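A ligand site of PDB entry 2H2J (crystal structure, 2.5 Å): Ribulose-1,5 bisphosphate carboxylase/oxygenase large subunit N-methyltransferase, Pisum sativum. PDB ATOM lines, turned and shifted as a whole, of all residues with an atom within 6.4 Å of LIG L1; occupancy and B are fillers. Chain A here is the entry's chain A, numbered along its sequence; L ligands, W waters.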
ATOM      1  N   SER A 173     -18.247  20.236  -9.794  1.00  0.00           N
ATOM      2  CA  SER A 173     -18.700  19.146  -8.936  1.00  0.00           C
ATOM      3  C   SER A 173     -19.516  18.129  -9.709  1.00  0.00           C
ATOM      4  O   SER A 173     -19.865  17.069  -9.163  1.00  0.00           O
ATOM      5  CB  SER A 173     -19.533  19.702  -7.768  1.00  0.00           C
ATOM      6  OG  SER A 173     -20.784  20.214  -8.193  1.00  0.00           O
ATOM      7  N   ARG A 174     -19.787  18.416 -10.976  1.00  0.00           N
ATOM      8  CA  ARG A 174     -20.596  17.525 -11.804  1.00  0.00           C
ATOM      9  C   ARG A 174     -19.956  16.955 -13.068  1.00  0.00           C
ATOM     10  O   ARG A 174     -20.123  15.764 -13.356  1.00  0.00           O
ATOM     11  CB  ARG A 174     -21.883  18.237 -12.170  1.00  0.00           C
ATOM     12  CG  ARG A 174     -22.785  18.427 -10.977  1.00  0.00           C
ATOM     13  CD  ARG A 174     -23.972  19.307 -11.287  1.00  0.00           C
ATOM     14  NE  ARG A 174     -25.062  19.017 -10.370  1.00  0.00           N
ATOM     15  CZ  ARG A 174     -25.786  17.910 -10.410  1.00  0.00           C
ATOM     16  NH1 ARG A 174     -25.538  16.995 -11.332  1.00  0.00           N
ATOM     17  NH2 ARG A 174     -26.772  17.715  -9.537  1.00  0.00           N
ATOM     18  N   ALA A 175     -19.250  17.783 -13.811  1.00  0.00           N
ATOM     19  CA  ALA A 175     -18.620  17.362 -15.060  1.00  0.00           C
ATOM     20  C   ALA A 175     -17.664  16.181 -14.890  1.00  0.00           C
ATOM     21  O   ALA A 175     -17.196  15.910 -13.789  1.00  0.00           O
ATOM     22  CB  ALA A 175     -17.880  18.536 -15.679  1.00  0.00           C
ATOM     23  N   PHE A 176     -17.373  15.504 -15.990  1.00  0.00           N
ATOM     24  CA  PHE A 176     -16.461  14.359 -15.983  1.00  0.00           C
ATOM     25  C   PHE A 176     -15.163  14.741 -16.680  1.00  0.00           C
ATOM     26  O   PHE A 176     -15.169  15.148 -17.839  1.00  0.00           O
ATOM     27  CB  PHE A 176     -17.082  13.161 -16.691  1.00  0.00           C
ATOM     28  CG  PHE A 176     -18.352  12.666 -16.055  1.00  0.00           C
ATOM     29  CD1 PHE A 176     -19.533  13.405 -16.150  1.00  0.00           C
ATOM     30  CD2 PHE A 176     -18.377  11.470 -15.355  1.00  0.00           C
ATOM     31  CE1 PHE A 176     -20.722  12.953 -15.560  1.00  0.00           C
ATOM     32  CE2 PHE A 176     -19.557  11.004 -14.765  1.00  0.00           C
ATOM     33  CZ  PHE A 176     -20.730  11.748 -14.872  1.00  0.00           C
ATOM     34  N   SER A 177     -14.071  14.605 -15.962  1.00  0.00           N
ATOM     35  CA  SER A 177     -12.745  14.947 -16.483  1.00  0.00           C
ATOM     36  C   SER A 177     -12.237  13.927 -17.497  1.00  0.00           C
ATOM     37  O   SER A 177     -12.374  14.108 -18.704  1.00  0.00           O
ATOM     38  CB  SER A 177     -11.747  15.088 -15.335  1.00  0.00           C
ATOM     39  OG  SER A 177     -12.183  16.041 -14.378  1.00  0.00           O
ATOM     40  N   ARG A 178     -11.635  12.858 -16.989  1.00  0.00           N
ATOM     41  CA  ARG A 178     -11.080  11.811 -17.837  1.00  0.00           C
ATOM     42  C   ARG A 178     -12.076  11.237 -18.840  1.00  0.00           C
ATOM     43  O   ARG A 178     -13.142  10.756 -18.471  1.00  0.00           O
ATOM     44  CB  ARG A 178     -10.494  10.688 -16.972  1.00  0.00           C
ATOM     45  CG  ARG A 178      -9.160  11.076 -16.316  1.00  0.00           C
ATOM     46  CD  ARG A 178      -8.623  10.016 -15.357  1.00  0.00           C
ATOM     47  NE  ARG A 178      -9.376   9.928 -14.100  1.00  0.00           N
ATOM     48  CZ  ARG A 178     -10.527   9.293 -13.958  1.00  0.00           C
ATOM     49  NH1 ARG A 178     -11.079   8.650 -14.988  1.00  0.00           N
ATOM     50  NH2 ARG A 178     -11.146   9.279 -12.781  1.00  0.00           N
ATOM     51  N   LEU A 179     -11.702  11.313 -20.120  1.00  0.00           N
ATOM     52  CA  LEU A 179     -12.508  10.812 -21.222  1.00  0.00           C
ATOM     53  C   LEU A 179     -11.634  10.062 -22.222  1.00  0.00           C
ATOM     54  O   LEU A 179     -10.868  10.672 -22.981  1.00  0.00           O
ATOM     55  CB  LEU A 179     -13.222  11.962 -21.940  1.00  0.00           C
ATOM     56  CG  LEU A 179     -14.677  12.245 -21.555  1.00  0.00           C
ATOM     57  CD1 LEU A 179     -15.491  10.964 -21.745  1.00  0.00           C
ATOM     58  CD2 LEU A 179     -14.752  12.742 -20.122  1.00  0.00           C
ATOM     59  N   ALA A 190     -26.149  10.880 -15.674  1.00  0.00           N
ATOM     60  CA  ALA A 190     -24.984  10.477 -14.898  1.00  0.00           C
ATOM     61  C   ALA A 190     -24.606  11.525 -13.837  1.00  0.00           C
ATOM     62  O   ALA A 190     -23.832  11.253 -12.921  1.00  0.00           O
ATOM     63  CB  ALA A 190     -23.806  10.250 -15.842  1.00  0.00           C
ATOM     64  N   ASP A 191     -25.179  12.720 -13.970  1.00  0.00           N
ATOM     65  CA  ASP A 191     -24.921  13.807 -13.045  1.00  0.00           C
ATOM     66  C   ASP A 191     -25.535  13.532 -11.672  1.00  0.00           C
ATOM     67  O   ASP A 191     -25.411  14.342 -10.766  1.00  0.00           O
ATOM     68  CB  ASP A 191     -25.539  15.106 -13.593  1.00  0.00           C
ATOM     69  CG  ASP A 191     -24.492  16.110 -14.014  1.00  0.00           C
ATOM     70  OD1 ASP A 191     -23.720  15.832 -14.962  1.00  0.00           O
ATOM     71  OD2 ASP A 191     -24.440  17.200 -13.407  1.00  0.00           O
ATOM     72  N   LEU A 192     -26.181  12.384 -11.515  1.00  0.00           N
ATOM     73  CA  LEU A 192     -26.835  12.054 -10.253  1.00  0.00           C
ATOM     74  C   LEU A 192     -26.132  11.014  -9.395  1.00  0.00           C
ATOM     75  O   LEU A 192     -26.374  10.940  -8.194  1.00  0.00           O
ATOM     76  CB  LEU A 192     -28.263  11.607 -10.532  1.00  0.00           C
ATOM     77  CG  LEU A 192     -29.101  12.670 -11.230  1.00  0.00           C
ATOM     78  CD1 LEU A 192     -30.447  12.099 -11.594  1.00  0.00           C
ATOM     79  CD2 LEU A 192     -29.261  13.866 -10.297  1.00  0.00           C
ATOM     80  N   ILE A 193     -25.285  10.196 -10.008  1.00  0.00           N
ATOM     81  CA  ILE A 193     -24.569   9.174  -9.267  1.00  0.00           C
ATOM     82  C   ILE A 193     -23.561   9.799  -8.296  1.00  0.00           C
ATOM     83  O   ILE A 193     -22.737  10.640  -8.669  1.00  0.00           O
ATOM     84  CB  ILE A 193     -23.848   8.225 -10.228  1.00  0.00           C
ATOM     85  CG1 ILE A 193     -23.242   7.055  -9.452  1.00  0.00           C
ATOM     86  CG2 ILE A 193     -22.760   8.975 -10.958  1.00  0.00           C
ATOM     87  CD1 ILE A 193     -22.661   5.992 -10.344  1.00  0.00           C
ATOM     88  N   ASN A 194     -23.644   9.384  -7.026  1.00  0.00           N
ATOM     89  CA  ASN A 194     -22.757   9.923  -5.999  1.00  0.00           C
ATOM     90  C   ASN A 194     -21.450   9.144  -5.810  1.00  0.00           C
ATOM     91  O   ASN A 194     -21.194   8.108  -6.453  1.00  0.00           O
ATOM     92  CB  ASN A 194     -23.504  10.000  -4.683  1.00  0.00           C
ATOM     93  CG  ASN A 194     -24.596  11.019  -4.705  1.00  0.00           C
ATOM     94  OD1 ASN A 194     -24.349  12.191  -4.917  1.00  0.00           O
ATOM     95  ND2 ASN A 194     -25.818  10.580  -4.483  1.00  0.00           N
ATOM     96  N   GLU A 202     -12.139   3.178  -9.998  1.00  0.00           N
ATOM     97  CA  GLU A 202     -12.121   4.434 -10.755  1.00  0.00           C
ATOM     98  C   GLU A 202     -11.902   4.222 -12.267  1.00  0.00           C
ATOM     99  O   GLU A 202     -10.767   4.104 -12.737  1.00  0.00           O
ATOM    100  CB  GLU A 202     -11.035   5.348 -10.201  1.00  0.00           C
ATOM    101  CG  GLU A 202     -11.031   6.758 -10.773  1.00  0.00           C
ATOM    102  CD  GLU A 202      -9.902   7.596 -10.209  1.00  0.00           C
ATOM    103  OE1 GLU A 202      -9.881   7.813  -8.984  1.00  0.00           O
ATOM    104  OE2 GLU A 202      -9.036   8.044 -10.998  1.00  0.00           O
ATOM    105  N   HIS A 204     -15.269   4.561 -15.162  1.00  0.00           N
ATOM    106  CA  HIS A 204     -16.654   4.280 -15.518  1.00  0.00           C
ATOM    107  C   HIS A 204     -17.106   5.066 -16.752  1.00  0.00           C
ATOM    108  O   HIS A 204     -18.272   5.003 -17.143  1.00  0.00           O
ATOM    109  CB  HIS A 204     -17.562   4.627 -14.329  1.00  0.00           C
ATOM    110  CG  HIS A 204     -16.843   4.662 -13.026  1.00  0.00           C
ATOM    111  ND1 HIS A 204     -16.316   3.531 -12.423  1.00  0.00           N
ATOM    112  CD2 HIS A 204     -16.518   5.700 -12.206  1.00  0.00           C
ATOM    113  CE1 HIS A 204     -15.703   3.869 -11.306  1.00  0.00           C
ATOM    114  NE2 HIS A 204     -15.810   5.181 -11.148  1.00  0.00           N
ATOM    115  N   ILE A 237     -19.777   5.474  -7.388  1.00  0.00           N
ATOM    116  CA  ILE A 237     -18.544   5.481  -8.168  1.00  0.00           C
ATOM    117  C   ILE A 237     -17.483   6.260  -7.397  1.00  0.00           C
ATOM    118  O   ILE A 237     -17.788   6.994  -6.466  1.00  0.00           O
ATOM    119  CB  ILE A 237     -18.716   6.156  -9.530  1.00  0.00           C
ATOM    120  CG1 ILE A 237     -19.372   7.526  -9.343  1.00  0.00           C
ATOM    121  CG2 ILE A 237     -19.507   5.260 -10.455  1.00  0.00           C
ATOM    122  CD1 ILE A 237     -19.273   8.417 -10.559  1.00  0.00           C
ATOM    123  N   GLN A 238     -16.235   6.093  -7.811  1.00  0.00           N
ATOM    124  CA  GLN A 238     -15.102   6.764  -7.187  1.00  0.00           C
ATOM    125  C   GLN A 238     -14.782   8.006  -7.987  1.00  0.00           C
ATOM    126  O   GLN A 238     -14.420   7.902  -9.160  1.00  0.00           O
ATOM    127  CB  GLN A 238     -13.896   5.833  -7.180  1.00  0.00           C
ATOM    128  CG  GLN A 238     -12.580   6.517  -6.854  1.00  0.00           C
ATOM    129  CD  GLN A 238     -12.635   7.207  -5.534  1.00  0.00           C
ATOM    130  OE1 GLN A 238     -12.942   6.597  -4.523  1.00  0.00           O
ATOM    131  NE2 GLN A 238     -12.326   8.490  -5.518  1.00  0.00           N
ATOM    132  N   TYR A 239     -14.917   9.176  -7.379  1.00  0.00           N
ATOM    133  CA  TYR A 239     -14.613  10.399  -8.100  1.00  0.00           C
ATOM    134  C   TYR A 239     -13.128  10.545  -8.417  1.00  0.00           C
ATOM    135  O   TYR A 239     -12.766  10.878  -9.545  1.00  0.00           O
ATOM    136  CB  TYR A 239     -15.110  11.615  -7.319  1.00  0.00           C
ATOM    137  CG  TYR A 239     -16.615  11.794  -7.339  1.00  0.00           C
ATOM    138  CD1 TYR A 239     -17.204  12.928  -6.783  1.00  0.00           C
ATOM    139  CD2 TYR A 239     -17.453  10.828  -7.908  1.00  0.00           C
ATOM    140  CE1 TYR A 239     -18.600  13.112  -6.796  1.00  0.00           C
ATOM    141  CE2 TYR A 239     -18.842  10.989  -7.926  1.00  0.00           C
ATOM    142  CZ  TYR A 239     -19.408  12.140  -7.367  1.00  0.00           C
ATOM    143  OH  TYR A 239     -20.775  12.309  -7.387  1.00  0.00           O
ATOM    144  N   ASP A 240     -12.267  10.297  -7.438  1.00  0.00           N
ATOM    145  CA  ASP A 240     -10.820  10.422  -7.645  1.00  0.00           C
ATOM    146  C   ASP A 240     -10.030   9.894  -6.445  1.00  0.00           C
ATOM    147  O   ASP A 240     -10.166  10.384  -5.334  1.00  0.00           O
ATOM    148  CB  ASP A 240     -10.445  11.883  -7.916  1.00  0.00           C
ATOM    149  CG  ASP A 240      -8.963  12.048  -8.244  1.00  0.00           C
ATOM    150  OD1 ASP A 240      -8.123  11.718  -7.377  1.00  0.00           O
ATOM    151  OD2 ASP A 240      -8.653  12.514  -9.353  1.00  0.00           O
ATOM    152  N   LYS A 243      -7.064  12.662  -5.045  1.00  0.00           N
ATOM    153  CA  LYS A 243      -7.318  13.968  -4.457  1.00  0.00           C
ATOM    154  C   LYS A 243      -7.182  13.920  -2.935  1.00  0.00           C
ATOM    155  O   LYS A 243      -7.407  12.889  -2.310  1.00  0.00           O
ATOM    156  CB  LYS A 243      -8.712  14.464  -4.835  1.00  0.00           C
ATOM    157  CG  LYS A 243      -8.819  14.961  -6.263  1.00  0.00           C
ATOM    158  CD  LYS A 243     -10.242  15.338  -6.649  1.00  0.00           C
ATOM    159  CE  LYS A 243     -10.280  16.023  -8.023  1.00  0.00           C
ATOM    160  NZ  LYS A 243     -11.690  16.340  -8.454  1.00  0.00           N
ATOM    161  N   TYR A 252     -16.040  19.240  -4.559  1.00  0.00           N
ATOM    162  CA  TYR A 252     -17.386  18.789  -4.206  1.00  0.00           C
ATOM    163  C   TYR A 252     -17.542  19.293  -2.791  1.00  0.00           C
ATOM    164  O   TYR A 252     -16.622  19.914  -2.256  1.00  0.00           O
ATOM    165  CB  TYR A 252     -17.469  17.264  -4.247  1.00  0.00           C
ATOM    166  CG  TYR A 252     -16.721  16.655  -5.410  1.00  0.00           C
ATOM    167  CD1 TYR A 252     -15.471  16.069  -5.222  1.00  0.00           C
ATOM    168  CD2 TYR A 252     -17.221  16.739  -6.703  1.00  0.00           C
ATOM    169  CE1 TYR A 252     -14.731  15.579  -6.302  1.00  0.00           C
ATOM    170  CE2 TYR A 252     -16.494  16.255  -7.788  1.00  0.00           C
ATOM    171  CZ  TYR A 252     -15.243  15.675  -7.571  1.00  0.00           C
ATOM    172  OH  TYR A 252     -14.503  15.208  -8.649  1.00  0.00           O
HETATM  173  N1  LIG L   1     -13.827  14.201 -12.230  1.00  0.00           N
HETATM  174  C1  LIG L   1     -14.080  12.836 -11.771  1.00  0.00           C
HETATM  175  C2  LIG L   1     -15.411  12.796 -10.995  1.00  0.00           C
HETATM  176  C3  LIG L   1     -16.615  13.335 -11.743  1.00  0.00           C
HETATM  177  C4  LIG L   1     -17.869  13.255 -10.893  1.00  0.00           C
HETATM  178  C5  LIG L   1     -19.122  13.218 -11.751  1.00  0.00           C
HETATM  179  N2  LIG L   1     -20.270  13.880 -11.072  1.00  0.00           N
HETATM  180  C6  LIG L   1     -21.569  13.322 -11.517  1.00  0.00           C
HETATM  181  C7  LIG L   1     -14.122  11.828 -12.938  1.00  0.00           C
HETATM  182  O1  LIG L   1     -13.951  12.246 -14.109  1.00  0.00           O
HETATM  183  O2  LIG L   1     -14.327  10.620 -12.663  1.00  0.00           O
HETATM  184  N1  LG2 L   2     -26.506  13.739  -5.988  1.00  0.00           N
HETATM  185  C1  LG2 L   2     -26.263  15.143  -6.268  1.00  0.00           C
HETATM  186  C2  LG2 L   2     -27.574  15.959  -6.319  1.00  0.00           C
HETATM  187  O1  LG2 L   2     -27.632  16.970  -7.054  1.00  0.00           O
HETATM  188  O2  LG2 L   2     -28.527  15.572  -5.636  1.00  0.00           O
HETATM  189  C3  LG2 L   2     -25.491  15.331  -7.601  1.00  0.00           C
HETATM  190  C4  LG2 L   2     -24.183  14.568  -7.837  1.00  0.00           C
HETATM  191  C5  LG2 L   2     -22.922  15.404  -8.203  1.00  0.00           C
HETATM  192  N2  LG2 L   2     -21.844  14.424  -8.500  1.00  0.00           N
HETATM  193  C6  LG2 L   2     -22.296  16.251  -7.047  1.00  0.00           C
HETATM  194  C7  LG2 L   2     -22.964  16.432  -5.698  1.00  0.00           C
HETATM  195  O3  LG2 L   2     -23.293  15.214  -5.016  1.00  0.00           O
HETATM  196  C8  LG2 L   2     -22.133  17.301  -4.743  1.00  0.00           C
HETATM  197  O4  LG2 L   2     -22.740  18.584  -4.530  1.00  0.00           O
HETATM  198  C9  LG2 L   2     -22.048  16.559  -3.473  1.00  0.00           C
HETATM  199  O5  LG2 L   2     -22.580  17.399  -2.447  1.00  0.00           O
HETATM  200  C10 LG2 L   2     -22.896  15.296  -3.640  1.00  0.00           C
HETATM  201  N3  LG2 L   2     -22.145  14.073  -3.234  1.00  0.00           N
HETATM  202  C11 LG2 L   2     -21.564  13.099  -4.015  1.00  0.00           C
HETATM  203  N4  LG2 L   2     -20.953  12.119  -3.400  1.00  0.00           N
HETATM  204  C12 LG2 L   2     -21.146  12.464  -2.044  1.00  0.00           C
HETATM  205  C13 LG2 L   2     -20.739  11.865  -0.806  1.00  0.00           C
HETATM  206  N5  LG2 L   2     -20.046  10.728  -0.760  1.00  0.00           N
HETATM  207  N6  LG2 L   2     -21.093  12.482   0.361  1.00  0.00           N
HETATM  208  C14 LG2 L   2     -21.796  13.647   0.312  1.00  0.00           C
HETATM  209  N7  LG2 L   2     -22.234  14.307  -0.775  1.00  0.00           N
HETATM  210  C15 LG2 L   2     -21.867  13.671  -1.934  1.00  0.00           C
HETATM  211  O   HOH W   1     -14.601  16.455 -13.457  1.00  0.00           O
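OD2 of Asp 191 is in salt-bridge range of NE of Arg 174 (3.6 Å). The side-chain hydroxyl (OH) of Tyr 252 sits at hydrogen-bond distance from the side-chain amino group (NZ) of Lys 243 (3.0 Å). The backbone carbonyl oxygen (O) of Ile 193 sits at hydrogen-bond distance from the side-chain hydroxyl (OH) of Tyr 239 (2.9 Å). The side-chain carboxylate (OE2) of Glu 202 is in salt-bridge range of the guanidinium group (NH2) of Arg 178.
Water W1 lies within hydrogen-bond range of OG of Ser 177 (2.6 Å), O of Ala 175 (2.7 Å) and N1 of LIG L1 (2.7 Å).
The backbone carbonyl oxygen (O) of Tyr 239 lies close to an oxygen (O2) of LIG L1 (3.5 Å). Residues that only touch LIG L1: Ala 175 (3.3 Å), Ala 190 (3.4 Å), Tyr 252 (3.5 Å), Asp 191 (3.7 Å), Ser 173 (3.7 Å) and Phe 176 (3.8 Å). Hydrophobic or aromatic side chains within 4 Å of LIG L1: Phe 176 and Tyr 239. Along chain A the residues within 4 Å of LIG L1 span positions 173 to 252.
N2 of LIG L1 lies close to N2 of LG2 L2.
The side-chain hydroxyl of Ser 177 lies within hydrogen-bond range of a nitrogen (N1) of LIG L1. NH2 of Arg 178 is in salt-bridge range of O2 of LIG L1, at 3.5 Å. O of Arg 174 is in hydrogen-bond range of N2 of LIG L1, at 3.0 Å. NH2 of Arg 174 lies within salt-bridge range of O1 of LG2 L2, at 2.7 Å. A nitrogen (N2) of LG2 L2 sits at hydrogen-bond distance from the side-chain hydroxyl (OH) of Tyr 239 (2.6 Å). N of Ser 177 is in hydrogen-bond range of O1 of LIG L1, at 3.0 Å. OD1 of Asn 194 lies within hydrogen-bond range of N1 of LG2 L2, at 2.9 Å. N2 of LG2 L2 lies close to O of Ser 173 (3.4 Å).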
